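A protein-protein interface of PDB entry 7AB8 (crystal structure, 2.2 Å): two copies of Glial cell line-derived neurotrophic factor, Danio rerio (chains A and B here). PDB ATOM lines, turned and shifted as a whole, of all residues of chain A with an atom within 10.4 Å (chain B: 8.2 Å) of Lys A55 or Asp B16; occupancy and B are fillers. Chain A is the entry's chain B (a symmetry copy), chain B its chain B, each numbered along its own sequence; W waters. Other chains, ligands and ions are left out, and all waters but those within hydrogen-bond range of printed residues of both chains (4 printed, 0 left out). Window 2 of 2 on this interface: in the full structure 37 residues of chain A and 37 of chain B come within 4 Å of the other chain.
The backbone carbonyl oxygen (O) of Asp B16 sits at hydrogen-bond distance from the side-chain amide nitrogen (ND2) of Asn A53 (3.0 Å). OD2 of Asp B16 is in salt-bridge range of NZ of Lys A55, at 3.99 Å. O of Leu B17 is in hydrogen-bond range of ND2 of Asn A49. The backbone carbonyl oxygen (O) of Asp B18 sits at hydrogen-bond distance from the side-chain amide nitrogen (ND2) of Asn A49, at 3.3 Å. OD2 of Asp B18 lies within hydrogen-bond range of ND2 of Asn A53, 2.8 Å away. The side-chain hydroxyl (OH) of Tyr B31 sits at hydrogen-bond distance from the side-chain carboxylate (OD2) of Asp A59, 2.7 Å away.
Among the printed residues, pairs that only touch across the chains: Lys A55 with Ile B10, Pro A61 with Tyr B31, Ile A46 with Phe B29, Leu A56 with Tyr B31, Leu A50 with Asp B16, Ile A46 with Leu B17, Leu A50 with Phe B29, Lys A55 with Leu B12, Leu A47 with Phe B29, Asn A49 with Leu B19 and Leu A50 with Leu B12.
Lys A55 touches three residues of chain B. Printed residues of chain A within 4 Å of Asp B16: Leu A50 (3.6 Å), Asn A53 (3.0 Å) and Lys A55 (3.8 Å). Of chain A, only Leu A50 and Lys A55 come within 4 Å of Leu B12. No residue of chain A comes within 4 Å of Thr B15. Leu B17 touches just these residues of chain A: Ile A46 (3.6 Å) and Asn A49 (2.7 Å). Of the printed residues of chain B, Asp A59 touches Tyr B31. Of the printed residues of chain A, Tyr B31 touches Leu A56, Asp A59 and Pro A61. Val B14 touches none of the printed residues of chain A. Thr A60 touches none of the printed residues of chain B. The nearest residue of chain B that does not touch Lys A55 is Asn B13 (6.2 Å). The nearest residue of chain A that does not touch Asp B16 is Asn A49 (5.2 Å). The nearest printed residue of chain B that does not touch Asp A59 is Ile B10 (8.0 Å).
Of the 18 printed residues of chain B, 8 touch a printed residue of chain A. Hydrophobic or aromatic side chains of chain B that line the printed part of chain A: Ile B10, Leu B12, Leu B17, Leu B19, Phe B29 and Tyr B31. Printed residues of chain A that touch a printed residue of chain B: Ile A46, Leu A47, Asn A49, Leu A50, Asn A53, Lys A55, Leu A56, Asp A59 and Pro A61. Along chain A the printed residues that touch a printed residue of chain B span positions 46 to 61. Among the printed residues, 17 pairs touch across the chains. Among the printed residues, Asp or Glu carboxylates within 4 Å of a Lys or Arg side-chain nitrogen of the other chain: Lys A55 with Asp B16.
Water W2 bridges OD2 of Asp B18 and O of Asn A49. Water W1 lies within hydrogen-bond range of the side-chain carboxylate of Asp B18 (2.9 Å), the side-chain amide nitrogen of Asn A53 (3.4 Å) and the backbone carbonyl oxygen of Thr B15 (3.5 Å). Water W4 lies within hydrogen-bond range of the side-chain amide nitrogen of Asn A49 and the backbone carbonyl oxygen of Asp B18.
No position is printed for both chains.
N of Ile B10 is in hydrogen-bond range of O of Phe B29 (2.9 Å). The backbone carbonyl oxygen of Leu B12 is in hydrogen-bond range of the backbone NH of Leu B27, at 3.0 Å. The side-chain carboxylate of Asp B16 lies within hydrogen-bond range of the backbone NH of Asn B13, at 2.9 Å. The backbone carbonyl oxygen of Lys A45 lies close to the side-chain amide oxygen of Asn A49 (3.5 Å). The backbone carbonyl oxygen (O) of Leu A50 lies within hydrogen-bond range of the backbone NH (N) of Lys A55.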
ATOM      1  N   ASN A  42     -18.808 -38.216  15.490  1.00  0.00           N
ATOM      2  CA  ASN A  42     -18.774 -37.060  16.380  1.00  0.00           C
ATOM      3  C   ASN A  42     -19.963 -36.147  16.128  1.00  0.00           C
ATOM      4  O   ASN A  42     -20.500 -35.550  17.069  1.00  0.00           O
ATOM      5  CB  ASN A  42     -17.469 -36.286  16.196  1.00  0.00           C
ATOM      6  CG  ASN A  42     -16.287 -36.966  16.858  1.00  0.00           C
ATOM      7  OD1 ASN A  42     -16.394 -37.473  17.973  1.00  0.00           O
ATOM      8  ND2 ASN A  42     -15.150 -36.972  16.173  1.00  0.00           N
ATOM      9  N   LYS A  45     -22.869 -37.539  18.052  1.00  0.00           N
ATOM     10  CA  LYS A  45     -22.660 -37.299  19.478  1.00  0.00           C
ATOM     11  C   LYS A  45     -22.900 -35.841  19.821  1.00  0.00           C
ATOM     12  O   LYS A  45     -23.541 -35.523  20.832  1.00  0.00           O
ATOM     13  CB  LYS A  45     -21.243 -37.704  19.881  1.00  0.00           C
ATOM     14  CG  LYS A  45     -20.841 -39.110  19.537  1.00  0.00           C
ATOM     15  CD  LYS A  45     -21.989 -40.076  19.631  1.00  0.00           C
ATOM     16  CE  LYS A  45     -21.438 -41.471  19.712  1.00  0.00           C
ATOM     17  NZ  LYS A  45     -22.250 -42.398  18.894  1.00  0.00           N
ATOM     18  N   ILE A  46     -22.371 -34.940  18.991  1.00  0.00           N
ATOM     19  CA  ILE A  46     -22.570 -33.512  19.209  1.00  0.00           C
ATOM     20  C   ILE A  46     -24.053 -33.167  19.172  1.00  0.00           C
ATOM     21  O   ILE A  46     -24.549 -32.396  20.005  1.00  0.00           O
ATOM     22  CB  ILE A  46     -21.772 -32.700  18.174  1.00  0.00           C
ATOM     23  CG1 ILE A  46     -20.280 -32.725  18.518  1.00  0.00           C
ATOM     24  CG2 ILE A  46     -22.272 -31.272  18.107  1.00  0.00           C
ATOM     25  CD1 ILE A  46     -19.373 -32.436  17.342  1.00  0.00           C
ATOM     26  N   LEU A  47     -24.785 -33.739  18.214  1.00  0.00           N
ATOM     27  CA  LEU A  47     -26.232 -33.561  18.174  1.00  0.00           C
ATOM     28  C   LEU A  47     -26.860 -33.948  19.507  1.00  0.00           C
ATOM     29  O   LEU A  47     -27.535 -33.137  20.147  1.00  0.00           O
ATOM     30  CB  LEU A  47     -26.837 -34.388  17.034  1.00  0.00           C
ATOM     31  CG  LEU A  47     -26.677 -33.857  15.609  1.00  0.00           C
ATOM     32  CD1 LEU A  47     -27.476 -34.707  14.634  1.00  0.00           C
ATOM     33  CD2 LEU A  47     -27.095 -32.398  15.522  1.00  0.00           C
ATOM     34  N   ASN A  48     -26.608 -35.183  19.953  1.00  0.00           N
ATOM     35  CA  ASN A  48     -27.173 -35.664  21.213  1.00  0.00           C
ATOM     36  C   ASN A  48     -26.847 -34.733  22.374  1.00  0.00           C
ATOM     37  O   ASN A  48     -27.699 -34.475  23.233  1.00  0.00           O
ATOM     38  CB  ASN A  48     -26.662 -37.075  21.505  1.00  0.00           C
ATOM     39  CG  ASN A  48     -27.190 -37.625  22.816  1.00  0.00           C
ATOM     40  OD1 ASN A  48     -26.420 -37.978  23.709  1.00  0.00           O
ATOM     41  ND2 ASN A  48     -28.510 -37.700  22.935  1.00  0.00           N
ATOM     42  N   ASN A  49     -25.619 -34.213  22.417  1.00  0.00           N
ATOM     43  CA  ASN A  49     -25.244 -33.320  23.507  1.00  0.00           C
ATOM     44  C   ASN A  49     -25.908 -31.956  23.372  1.00  0.00           C
ATOM     45  O   ASN A  49     -26.236 -31.329  24.385  1.00  0.00           O
ATOM     46  CB  ASN A  49     -23.725 -33.173  23.570  1.00  0.00           C
ATOM     47  CG  ASN A  49     -23.031 -34.468  23.940  1.00  0.00           C
ATOM     48  OD1 ASN A  49     -23.680 -35.455  24.285  1.00  0.00           O
ATOM     49  ND2 ASN A  49     -21.705 -34.472  23.870  1.00  0.00           N
ATOM     50  N   LEU A  50     -26.120 -31.483  22.142  1.00  0.00           N
ATOM     51  CA  LEU A  50     -26.734 -30.174  21.950  1.00  0.00           C
ATOM     52  C   LEU A  50     -28.242 -30.205  22.174  1.00  0.00           C
ATOM     53  O   LEU A  50     -28.816 -29.192  22.587  1.00  0.00           O
ATOM     54  CB  LEU A  50     -26.414 -29.636  20.554  1.00  0.00           C
ATOM     55  CG  LEU A  50     -24.957 -29.240  20.293  1.00  0.00           C
ATOM     56  CD1 LEU A  50     -24.782 -28.756  18.861  1.00  0.00           C
ATOM     57  CD2 LEU A  50     -24.480 -28.185  21.281  1.00  0.00           C
ATOM     58  N   THR A  51     -28.902 -31.336  21.901  1.00  0.00           N
ATOM     59  CA  THR A  51     -30.302 -31.477  22.296  1.00  0.00           C
ATOM     60  C   THR A  51     -30.445 -31.347  23.805  1.00  0.00           C
ATOM     61  O   THR A  51     -31.271 -30.572  24.303  1.00  0.00           O
ATOM     62  CB  THR A  51     -30.871 -32.822  21.836  1.00  0.00           C
ATOM     63  OG1 THR A  51     -30.369 -33.870  22.677  1.00  0.00           O
ATOM     64  CG2 THR A  51     -30.521 -33.107  20.387  1.00  0.00           C
ATOM     65  N   HIS A  52     -29.641 -32.108  24.549  1.00  0.00           N
ATOM     66  CA  HIS A  52     -29.668 -32.035  26.004  1.00  0.00           C
ATOM     67  C   HIS A  52     -29.220 -30.668  26.505  1.00  0.00           C
ATOM     68  O   HIS A  52     -29.638 -30.235  27.585  1.00  0.00           O
ATOM     69  CB  HIS A  52     -28.786 -33.141  26.587  1.00  0.00           C
ATOM     70  CG  HIS A  52     -28.789 -33.201  28.082  1.00  0.00           C
ATOM     71  ND1 HIS A  52     -28.202 -32.233  28.869  1.00  0.00           N
ATOM     72  CD2 HIS A  52     -29.300 -34.119  28.936  1.00  0.00           C
ATOM     73  CE1 HIS A  52     -28.358 -32.548  30.142  1.00  0.00           C
ATOM     74  NE2 HIS A  52     -29.019 -33.689  30.210  1.00  0.00           N
ATOM     75  N   ASN A  53     -28.379 -29.972  25.738  1.00  0.00           N
ATOM     76  CA  ASN A  53     -27.849 -28.679  26.153  1.00  0.00           C
ATOM     77  C   ASN A  53     -28.788 -27.518  25.861  1.00  0.00           C
ATOM     78  O   ASN A  53     -28.549 -26.417  26.371  1.00  0.00           O
ATOM     79  CB  ASN A  53     -26.510 -28.414  25.464  1.00  0.00           C
ATOM     80  CG  ASN A  53     -25.339 -28.514  26.413  1.00  0.00           C
ATOM     81  OD1 ASN A  53     -25.517 -28.582  27.628  1.00  0.00           O
ATOM     82  ND2 ASN A  53     -24.131 -28.514  25.864  1.00  0.00           N
ATOM     83  N   LYS A  54     -29.791 -27.772  25.034  1.00  0.00           N
ATOM     84  CA  LYS A  54     -30.771 -26.843  24.564  1.00  0.00           C
ATOM     85  C   LYS A  54     -30.081 -25.797  23.727  1.00  0.00           C
ATOM     86  O   LYS A  54     -30.613 -24.749  23.524  1.00  0.00           O
ATOM     87  CB  LYS A  54     -31.657 -26.207  25.668  1.00  0.00           C
ATOM     88  CG  LYS A  54     -32.615 -27.115  26.409  1.00  0.00           C
ATOM     89  CD  LYS A  54     -33.428 -26.421  27.488  1.00  0.00           C
ATOM     90  CE  LYS A  54     -34.373 -27.393  28.158  1.00  0.00           C
ATOM     91  NZ  LYS A  54     -35.158 -26.730  29.234  1.00  0.00           N
ATOM     92  N   LYS A  55     -28.934 -26.107  23.165  1.00  0.00           N
ATOM     93  CA  LYS A  55     -28.188 -25.112  22.452  1.00  0.00           C
ATOM     94  C   LYS A  55     -28.625 -24.975  21.013  1.00  0.00           C
ATOM     95  O   LYS A  55     -28.274 -24.038  20.357  1.00  0.00           O
ATOM     96  CB  LYS A  55     -26.719 -25.438  22.532  1.00  0.00           C
ATOM     97  CG  LYS A  55     -25.988 -24.903  23.746  1.00  0.00           C
ATOM     98  CD  LYS A  55     -25.336 -23.584  23.490  1.00  0.00           C
ATOM     99  CE  LYS A  55     -24.753 -23.025  24.762  1.00  0.00           C
ATOM    100  NZ  LYS A  55     -24.413 -21.612  24.557  1.00  0.00           N
ATOM    101  N   LEU A  56     -29.449 -25.879  20.536  1.00  0.00           N
ATOM    102  CA  LEU A  56     -29.924 -25.758  19.173  1.00  0.00           C
ATOM    103  C   LEU A  56     -31.357 -25.192  19.085  1.00  0.00           C
ATOM    104  O   LEU A  56     -32.000 -25.269  18.054  1.00  0.00           O
ATOM    105  CB  LEU A  56     -29.903 -27.121  18.515  1.00  0.00           C
ATOM    106  CG  LEU A  56     -28.586 -27.518  17.903  1.00  0.00           C
ATOM    107  CD1 LEU A  56     -28.677 -28.811  17.161  1.00  0.00           C
ATOM    108  CD2 LEU A  56     -28.047 -26.431  17.045  1.00  0.00           C
ATOM    109  N   ASP A  57     -31.800 -24.582  20.175  1.00  0.00           N
ATOM    110  CA  ASP A  57     -33.134 -24.025  20.249  1.00  0.00           C
ATOM    111  C   ASP A  57     -34.185 -25.129  19.898  1.00  0.00           C
ATOM    112  O   ASP A  57     -34.295 -26.068  20.686  1.00  0.00           O
ATOM    113  CB  ASP A  57     -33.224 -22.676  19.496  1.00  0.00           C
ATOM    114  CG  ASP A  57     -34.532 -21.953  19.751  1.00  0.00           C
ATOM    115  OD1 ASP A  57     -34.833 -21.665  20.928  1.00  0.00           O
ATOM    116  OD2 ASP A  57     -35.259 -21.673  18.774  1.00  0.00           O
ATOM    117  N   LYS A  58     -34.953 -25.090  18.802  1.00  0.00           N
ATOM    118  CA  LYS A  58     -35.967 -26.118  18.639  1.00  0.00           C
ATOM    119  C   LYS A  58     -35.677 -27.000  17.452  1.00  0.00           C
ATOM    120  O   LYS A  58     -36.591 -27.661  16.954  1.00  0.00           O
ATOM    121  CB  LYS A  58     -37.378 -25.558  18.429  1.00  0.00           C
ATOM    122  CG  LYS A  58     -38.057 -25.102  19.711  1.00  0.00           C
ATOM    123  CD  LYS A  58     -39.332 -24.326  19.422  1.00  0.00           C
ATOM    124  CE  LYS A  58     -39.930 -23.744  20.694  1.00  0.00           C
ATOM    125  NZ  LYS A  58     -41.205 -23.022  20.433  1.00  0.00           N
ATOM    126  N   ASP A  59     -34.441 -27.039  16.977  1.00  0.00           N
ATOM    127  CA  ASP A  59     -34.192 -27.905  15.888  1.00  0.00           C
ATOM    128  C   ASP A  59     -33.890 -29.216  16.571  1.00  0.00           C
ATOM    129  O   ASP A  59     -33.197 -29.216  17.547  1.00  0.00           O
ATOM    130  CB  ASP A  59     -33.015 -27.427  15.080  1.00  0.00           C
ATOM    131  CG  ASP A  59     -33.316 -26.184  14.312  1.00  0.00           C
ATOM    132  OD1 ASP A  59     -34.468 -25.870  14.190  1.00  0.00           O
ATOM    133  OD2 ASP A  59     -32.412 -25.536  13.820  1.00  0.00           O
ATOM    134  N   THR A  60     -34.426 -30.314  16.067  1.00  0.00           N
ATOM    135  CA  THR A  60     -34.151 -31.646  16.627  1.00  0.00           C
ATOM    136  C   THR A  60     -33.578 -32.457  15.448  1.00  0.00           C
ATOM    137  O   THR A  60     -34.227 -33.335  14.936  1.00  0.00           O
ATOM    138  CB  THR A  60     -35.345 -32.310  17.264  1.00  0.00           C
ATOM    139  OG1 THR A  60     -36.363 -32.464  16.283  1.00  0.00           O
ATOM    140  CG2 THR A  60     -35.855 -31.461  18.375  1.00  0.00           C
ATOM    141  N   PRO A  61     -32.261 -32.181  15.080  1.00  0.00           N
ATOM    142  CA  PRO A  61     -31.745 -32.860  13.888  1.00  0.00           C
ATOM    143  C   PRO A  61     -31.643 -34.362  14.104  1.00  0.00           C
ATOM    144  O   PRO A  61     -31.500 -34.846  15.229  1.00  0.00           O
ATOM    145  CB  PRO A  61     -30.361 -32.228  13.686  1.00  0.00           C
ATOM    146  CG  PRO A  61     -30.376 -30.978  14.513  1.00  0.00           C
ATOM    147  CD  PRO A  61     -31.258 -31.284  15.673  1.00  0.00           C
ATOM    148  N   ILE B  10     -24.201 -22.986  13.542  1.00  0.00           N
ATOM    149  CA  ILE B  10     -24.251 -22.253  14.802  1.00  0.00           C
ATOM    150  C   ILE B  10     -22.830 -22.084  15.321  1.00  0.00           C
ATOM    151  O   ILE B  10     -22.008 -23.003  15.239  1.00  0.00           O
ATOM    152  CB  ILE B  10     -25.159 -22.963  15.833  1.00  0.00           C
ATOM    153  CG1 ILE B  10     -25.281 -22.130  17.110  1.00  0.00           C
ATOM    154  CG2 ILE B  10     -24.650 -24.368  16.139  1.00  0.00           C
ATOM    155  CD1 ILE B  10     -26.184 -22.746  18.153  1.00  0.00           C
ATOM    156  N   HIS B  11     -22.539 -20.894  15.838  1.00  0.00           N
ATOM    157  CA  HIS B  11     -21.236 -20.583  16.412  1.00  0.00           C
ATOM    158  C   HIS B  11     -21.232 -21.003  17.878  1.00  0.00           C
ATOM    159  O   HIS B  11     -22.076 -20.550  18.659  1.00  0.00           O
ATOM    160  CB  HIS B  11     -20.933 -19.092  16.267  1.00  0.00           C
ATOM    161  CG  HIS B  11     -19.643 -18.667  16.897  1.00  0.00           C
ATOM    162  ND1 HIS B  11     -19.398 -17.365  17.278  1.00  0.00           N
ATOM    163  CD2 HIS B  11     -18.526 -19.366  17.206  1.00  0.00           C
ATOM    164  CE1 HIS B  11     -18.186 -17.281  17.798  1.00  0.00           C
ATOM    165  NE2 HIS B  11     -17.636 -18.482  17.767  1.00  0.00           N
ATOM    166  N   LEU B  12     -20.289 -21.865  18.248  1.00  0.00           N
ATOM    167  CA  LEU B  12     -20.248 -22.423  19.591  1.00  0.00           C
ATOM    168  C   LEU B  12     -18.820 -22.430  20.113  1.00  0.00           C
ATOM    169  O   LEU B  12     -17.852 -22.415  19.348  1.00  0.00           O
ATOM    170  CB  LEU B  12     -20.806 -23.853  19.628  1.00  0.00           C
ATOM    171  CG  LEU B  12     -22.274 -24.067  19.266  1.00  0.00           C
ATOM    172  CD1 LEU B  12     -22.536 -25.538  18.983  1.00  0.00           C
ATOM    173  CD2 LEU B  12     -23.178 -23.562  20.380  1.00  0.00           C
ATOM    174  N   ASN B  13     -18.703 -22.445  21.438  1.00  0.00           N
ATOM    175  CA  ASN B  13     -17.450 -22.816  22.072  1.00  0.00           C
ATOM    176  C   ASN B  13     -17.252 -24.324  21.949  1.00  0.00           C
ATOM    177  O   ASN B  13     -18.214 -25.088  21.828  1.00  0.00           O
ATOM    178  CB  ASN B  13     -17.448 -22.414  23.548  1.00  0.00           C
ATOM    179  CG  ASN B  13     -17.384 -20.909  23.757  1.00  0.00           C
ATOM    180  OD1 ASN B  13     -16.497 -20.231  23.241  1.00  0.00           O
ATOM    181  ND2 ASN B  13     -18.331 -20.385  24.531  1.00  0.00           N
ATOM    182  N   VAL B  14     -15.989 -24.756  21.976  1.00  0.00           N
ATOM    183  CA  VAL B  14     -15.718 -26.191  21.947  1.00  0.00           C
ATOM    184  C   VAL B  14     -16.304 -26.867  23.181  1.00  0.00           C
ATOM    185  O   VAL B  14     -16.770 -28.012  23.111  1.00  0.00           O
ATOM    186  CB  VAL B  14     -14.202 -26.450  21.816  1.00  0.00           C
ATOM    187  CG1 VAL B  14     -13.880 -27.918  22.063  1.00  0.00           C
ATOM    188  CG2 VAL B  14     -13.713 -26.031  20.438  1.00  0.00           C
ATOM    189  N   THR B  15     -16.325 -26.164  24.318  1.00  0.00           N
ATOM    190  CA  THR B  15     -16.893 -26.735  25.535  1.00  0.00           C
ATOM    191  C   THR B  15     -18.388 -26.995  25.397  1.00  0.00           C
ATOM    192  O   THR B  15     -18.925 -27.884  26.069  1.00  0.00           O
ATOM    193  CB  THR B  15     -16.632 -25.812  26.726  1.00  0.00           C
ATOM    194  OG1 THR B  15     -17.201 -24.523  26.467  1.00  0.00           O
ATOM    195  CG2 THR B  15     -15.140 -25.665  26.969  1.00  0.00           C
ATOM    196  N   ASP B  16     -19.075 -26.236  24.538  1.00  0.00           N
ATOM    197  CA  ASP B  16     -20.503 -26.455  24.329  1.00  0.00           C
ATOM    198  C   ASP B  16     -20.799 -27.838  23.763  1.00  0.00           C
ATOM    199  O   ASP B  16     -21.939 -28.303  23.855  1.00  0.00           O
ATOM    200  CB  ASP B  16     -21.074 -25.383  23.398  1.00  0.00           C
ATOM    201  CG  ASP B  16     -21.026 -23.994  24.005  1.00  0.00           C
ATOM    202  OD1 ASP B  16     -21.100 -23.882  25.247  1.00  0.00           O
ATOM    203  OD2 ASP B  16     -20.918 -23.015  23.239  1.00  0.00           O
ATOM    204  N   LEU B  17     -19.799 -28.502  23.179  1.00  0.00           N
ATOM    205  CA  LEU B  17     -20.004 -29.841  22.641  1.00  0.00           C
ATOM    206  C   LEU B  17     -20.096 -30.897  23.735  1.00  0.00           C
ATOM    207  O   LEU B  17     -20.581 -32.002  23.469  1.00  0.00           O
ATOM    208  CB  LEU B  17     -18.877 -30.194  21.670  1.00  0.00           C
ATOM    209  CG  LEU B  17     -18.632 -29.187  20.542  1.00  0.00           C
ATOM    210  CD1 LEU B  17     -17.431 -29.595  19.703  1.00  0.00           C
ATOM    211  CD2 LEU B  17     -19.872 -29.041  19.675  1.00  0.00           C
ATOM    212  N   ASP B  18     -19.639 -30.582  24.951  1.00  0.00           N
ATOM    213  CA  ASP B  18     -19.711 -31.493  26.095  1.00  0.00           C
ATOM    214  C   ASP B  18     -18.999 -32.813  25.808  1.00  0.00           C
ATOM    215  O   ASP B  18     -19.448 -33.886  26.216  1.00  0.00           O
ATOM    216  CB  ASP B  18     -21.163 -31.740  26.518  1.00  0.00           C
ATOM    217  CG  ASP B  18     -21.710 -30.630  27.394  1.00  0.00           C
ATOM    218  OD1 ASP B  18     -20.902 -29.901  28.007  1.00  0.00           O
ATOM    219  OD2 ASP B  18     -22.948 -30.485  27.470  1.00  0.00           O
ATOM    220  N   LEU B  19     -17.874 -32.736  25.100  1.00  0.00           N
ATOM    221  CA  LEU B  19     -17.078 -33.911  24.776  1.00  0.00           C
ATOM    222  C   LEU B  19     -15.905 -34.113  25.726  1.00  0.00           C
ATOM    223  O   LEU B  19     -15.101 -35.025  25.510  1.00  0.00           O
ATOM    224  CB  LEU B  19     -16.573 -33.823  23.332  1.00  0.00           C
ATOM    225  CG  LEU B  19     -17.656 -33.932  22.256  1.00  0.00           C
ATOM    226  CD1 LEU B  19     -17.103 -33.556  20.891  1.00  0.00           C
ATOM    227  CD2 LEU B  19     -18.254 -35.333  22.231  1.00  0.00           C
ATOM    228  N   GLY B  20     -15.790 -33.293  26.771  1.00  0.00           N
ATOM    229  CA  GLY B  20     -14.780 -33.472  27.792  1.00  0.00           C
ATOM    230  C   GLY B  20     -13.565 -32.579  27.662  1.00  0.00           C
ATOM    231  O   GLY B  20     -12.766 -32.512  28.605  1.00  0.00           O
ATOM    232  N   TYR B  21     -13.399 -31.897  26.533  1.00  0.00           N
ATOM    233  CA  TYR B  21     -12.235 -31.044  26.343  1.00  0.00           C
ATOM    234  C   TYR B  21     -12.336 -29.797  27.212  1.00  0.00           C
ATOM    235  O   TYR B  21     -13.423 -29.254  27.430  1.00  0.00           O
ATOM    236  CB  TYR B  21     -12.101 -30.650  24.872  1.00  0.00           C
ATOM    237  CG  TYR B  21     -12.052 -31.833  23.934  1.00  0.00           C
ATOM    238  CD1 TYR B  21     -10.907 -32.610  23.827  1.00  0.00           C
ATOM    239  CD2 TYR B  21     -13.154 -32.177  23.162  1.00  0.00           C
ATOM    240  CE1 TYR B  21     -10.858 -33.696  22.973  1.00  0.00           C
ATOM    241  CE2 TYR B  21     -13.114 -33.261  22.305  1.00  0.00           C
ATOM    242  CZ  TYR B  21     -11.963 -34.016  22.216  1.00  0.00           C
ATOM    243  OH  TYR B  21     -11.915 -35.097  21.367  1.00  0.00           O
ATOM    244  N   THR B  23     -10.954 -26.255  26.929  1.00  0.00           N
ATOM    245  CA  THR B  23     -10.307 -25.316  26.026  1.00  0.00           C
ATOM    246  C   THR B  23     -11.230 -24.127  25.822  1.00  0.00           C
ATOM    247  O   THR B  23     -12.443 -24.219  26.027  1.00  0.00           O
ATOM    248  CB  THR B  23      -9.970 -25.972  24.682  1.00  0.00           C
ATOM    249  OG1 THR B  23      -9.608 -24.964  23.730  1.00  0.00           O
ATOM    250  CG2 THR B  23     -11.170 -26.743  24.158  1.00  0.00           C
ATOM    251  N   GLU B  25     -11.198 -22.565  22.791  1.00  0.00           N
ATOM    252  CA  GLU B  25     -11.331 -22.442  21.349  1.00  0.00           C
ATOM    253  C   GLU B  25     -12.794 -22.578  20.934  1.00  0.00           C
ATOM    254  O   GLU B  25     -13.638 -23.078  21.683  1.00  0.00           O
ATOM    255  CB  GLU B  25     -10.471 -23.491  20.641  1.00  0.00           C
ATOM    256  CG  GLU B  25      -8.973 -23.268  20.809  1.00  0.00           C
ATOM    257  CD  GLU B  25      -8.190 -23.549  19.539  1.00  0.00           C
ATOM    258  OE1 GLU B  25      -8.790 -23.496  18.444  1.00  0.00           O
ATOM    259  OE2 GLU B  25      -6.976 -23.826  19.637  1.00  0.00           O
ATOM    260  N   GLU B  26     -13.089 -22.114  19.721  1.00  0.00           N
ATOM    261  CA  GLU B  26     -14.449 -22.068  19.202  1.00  0.00           C
ATOM    262  C   GLU B  26     -14.511 -22.792  17.861  1.00  0.00           C
ATOM    263  O   GLU B  26     -13.495 -23.235  17.317  1.00  0.00           O
ATOM    264  CB  GLU B  26     -14.940 -20.621  19.059  1.00  0.00           C
ATOM    265  CG  GLU B  26     -15.062 -19.877  20.373  1.00  0.00           C
ATOM    266  CD  GLU B  26     -15.390 -18.411  20.177  1.00  0.00           C
ATOM    267  OE1 GLU B  26     -15.507 -17.977  19.013  1.00  0.00           O
ATOM    268  OE2 GLU B  26     -15.497 -17.685  21.190  1.00  0.00           O
ATOM    269  N   LEU B  27     -15.726 -22.901  17.324  1.00  0.00           N
ATOM    270  CA  LEU B  27     -15.940 -23.597  16.065  1.00  0.00           C
ATOM    271  C   LEU B  27     -17.295 -23.205  15.496  1.00  0.00           C
ATOM    272  O   LEU B  27     -18.150 -22.654  16.194  1.00  0.00           O
ATOM    273  CB  LEU B  27     -15.865 -25.117  16.244  1.00  0.00           C
ATOM    274  CG  LEU B  27     -17.085 -25.807  16.856  1.00  0.00           C
ATOM    275  CD1 LEU B  27     -17.243 -27.209  16.289  1.00  0.00           C
ATOM    276  CD2 LEU B  27     -16.972 -25.850  18.371  1.00  0.00           C
ATOM    277  N   PHE B  29     -20.317 -25.186  14.045  1.00  0.00           N
ATOM    278  CA  PHE B  29     -20.928 -26.497  13.890  1.00  0.00           C
ATOM    279  C   PHE B  29     -22.062 -26.412  12.878  1.00  0.00           C
ATOM    280  O   PHE B  29     -22.953 -25.566  13.007  1.00  0.00           O
ATOM    281  CB  PHE B  29     -21.452 -27.018  15.230  1.00  0.00           C
ATOM    282  CG  PHE B  29     -22.249 -28.286  15.116  1.00  0.00           C
ATOM    283  CD1 PHE B  29     -21.638 -29.475  14.755  1.00  0.00           C
ATOM    284  CD2 PHE B  29     -23.611 -28.288  15.365  1.00  0.00           C
ATOM    285  CE1 PHE B  29     -22.369 -30.642  14.647  1.00  0.00           C
ATOM    286  CE2 PHE B  29     -24.349 -29.453  15.259  1.00  0.00           C
ATOM    287  CZ  PHE B  29     -23.726 -30.631  14.900  1.00  0.00           C
ATOM    288  N   TYR B  31     -25.089 -28.560  10.697  1.00  0.00           N
ATOM    289  CA  TYR B  31     -25.938 -29.734  10.818  1.00  0.00           C
ATOM    290  C   TYR B  31     -27.049 -29.670   9.781  1.00  0.00           C
ATOM    291  O   TYR B  31     -27.353 -28.609   9.229  1.00  0.00           O
ATOM    292  CB  TYR B  31     -26.536 -29.848  12.227  1.00  0.00           C
ATOM    293  CG  TYR B  31     -27.375 -28.660  12.645  1.00  0.00           C
ATOM    294  CD1 TYR B  31     -26.784 -27.511  13.157  1.00  0.00           C
ATOM    295  CD2 TYR B  31     -28.759 -28.689  12.535  1.00  0.00           C
ATOM    296  CE1 TYR B  31     -27.547 -26.425  13.541  1.00  0.00           C
ATOM    297  CE2 TYR B  31     -29.531 -27.609  12.920  1.00  0.00           C
ATOM    298  CZ  TYR B  31     -28.920 -26.481  13.422  1.00  0.00           C
ATOM    299  OH  TYR B  31     -29.687 -25.404  13.804  1.00  0.00           O
HETATM  300  O   HOH W   1     -21.795 -27.126  27.865  1.00  0.00           O
HETATM  301  O   HOH W   2     -24.868 -32.110  26.872  1.00  0.00           O
HETATM  302  O   HOH W   3     -23.664 -28.936  29.643  1.00  0.00           O
HETATM  303  O   HOH W   4     -20.721 -36.976  25.347  1.00  0.00           O
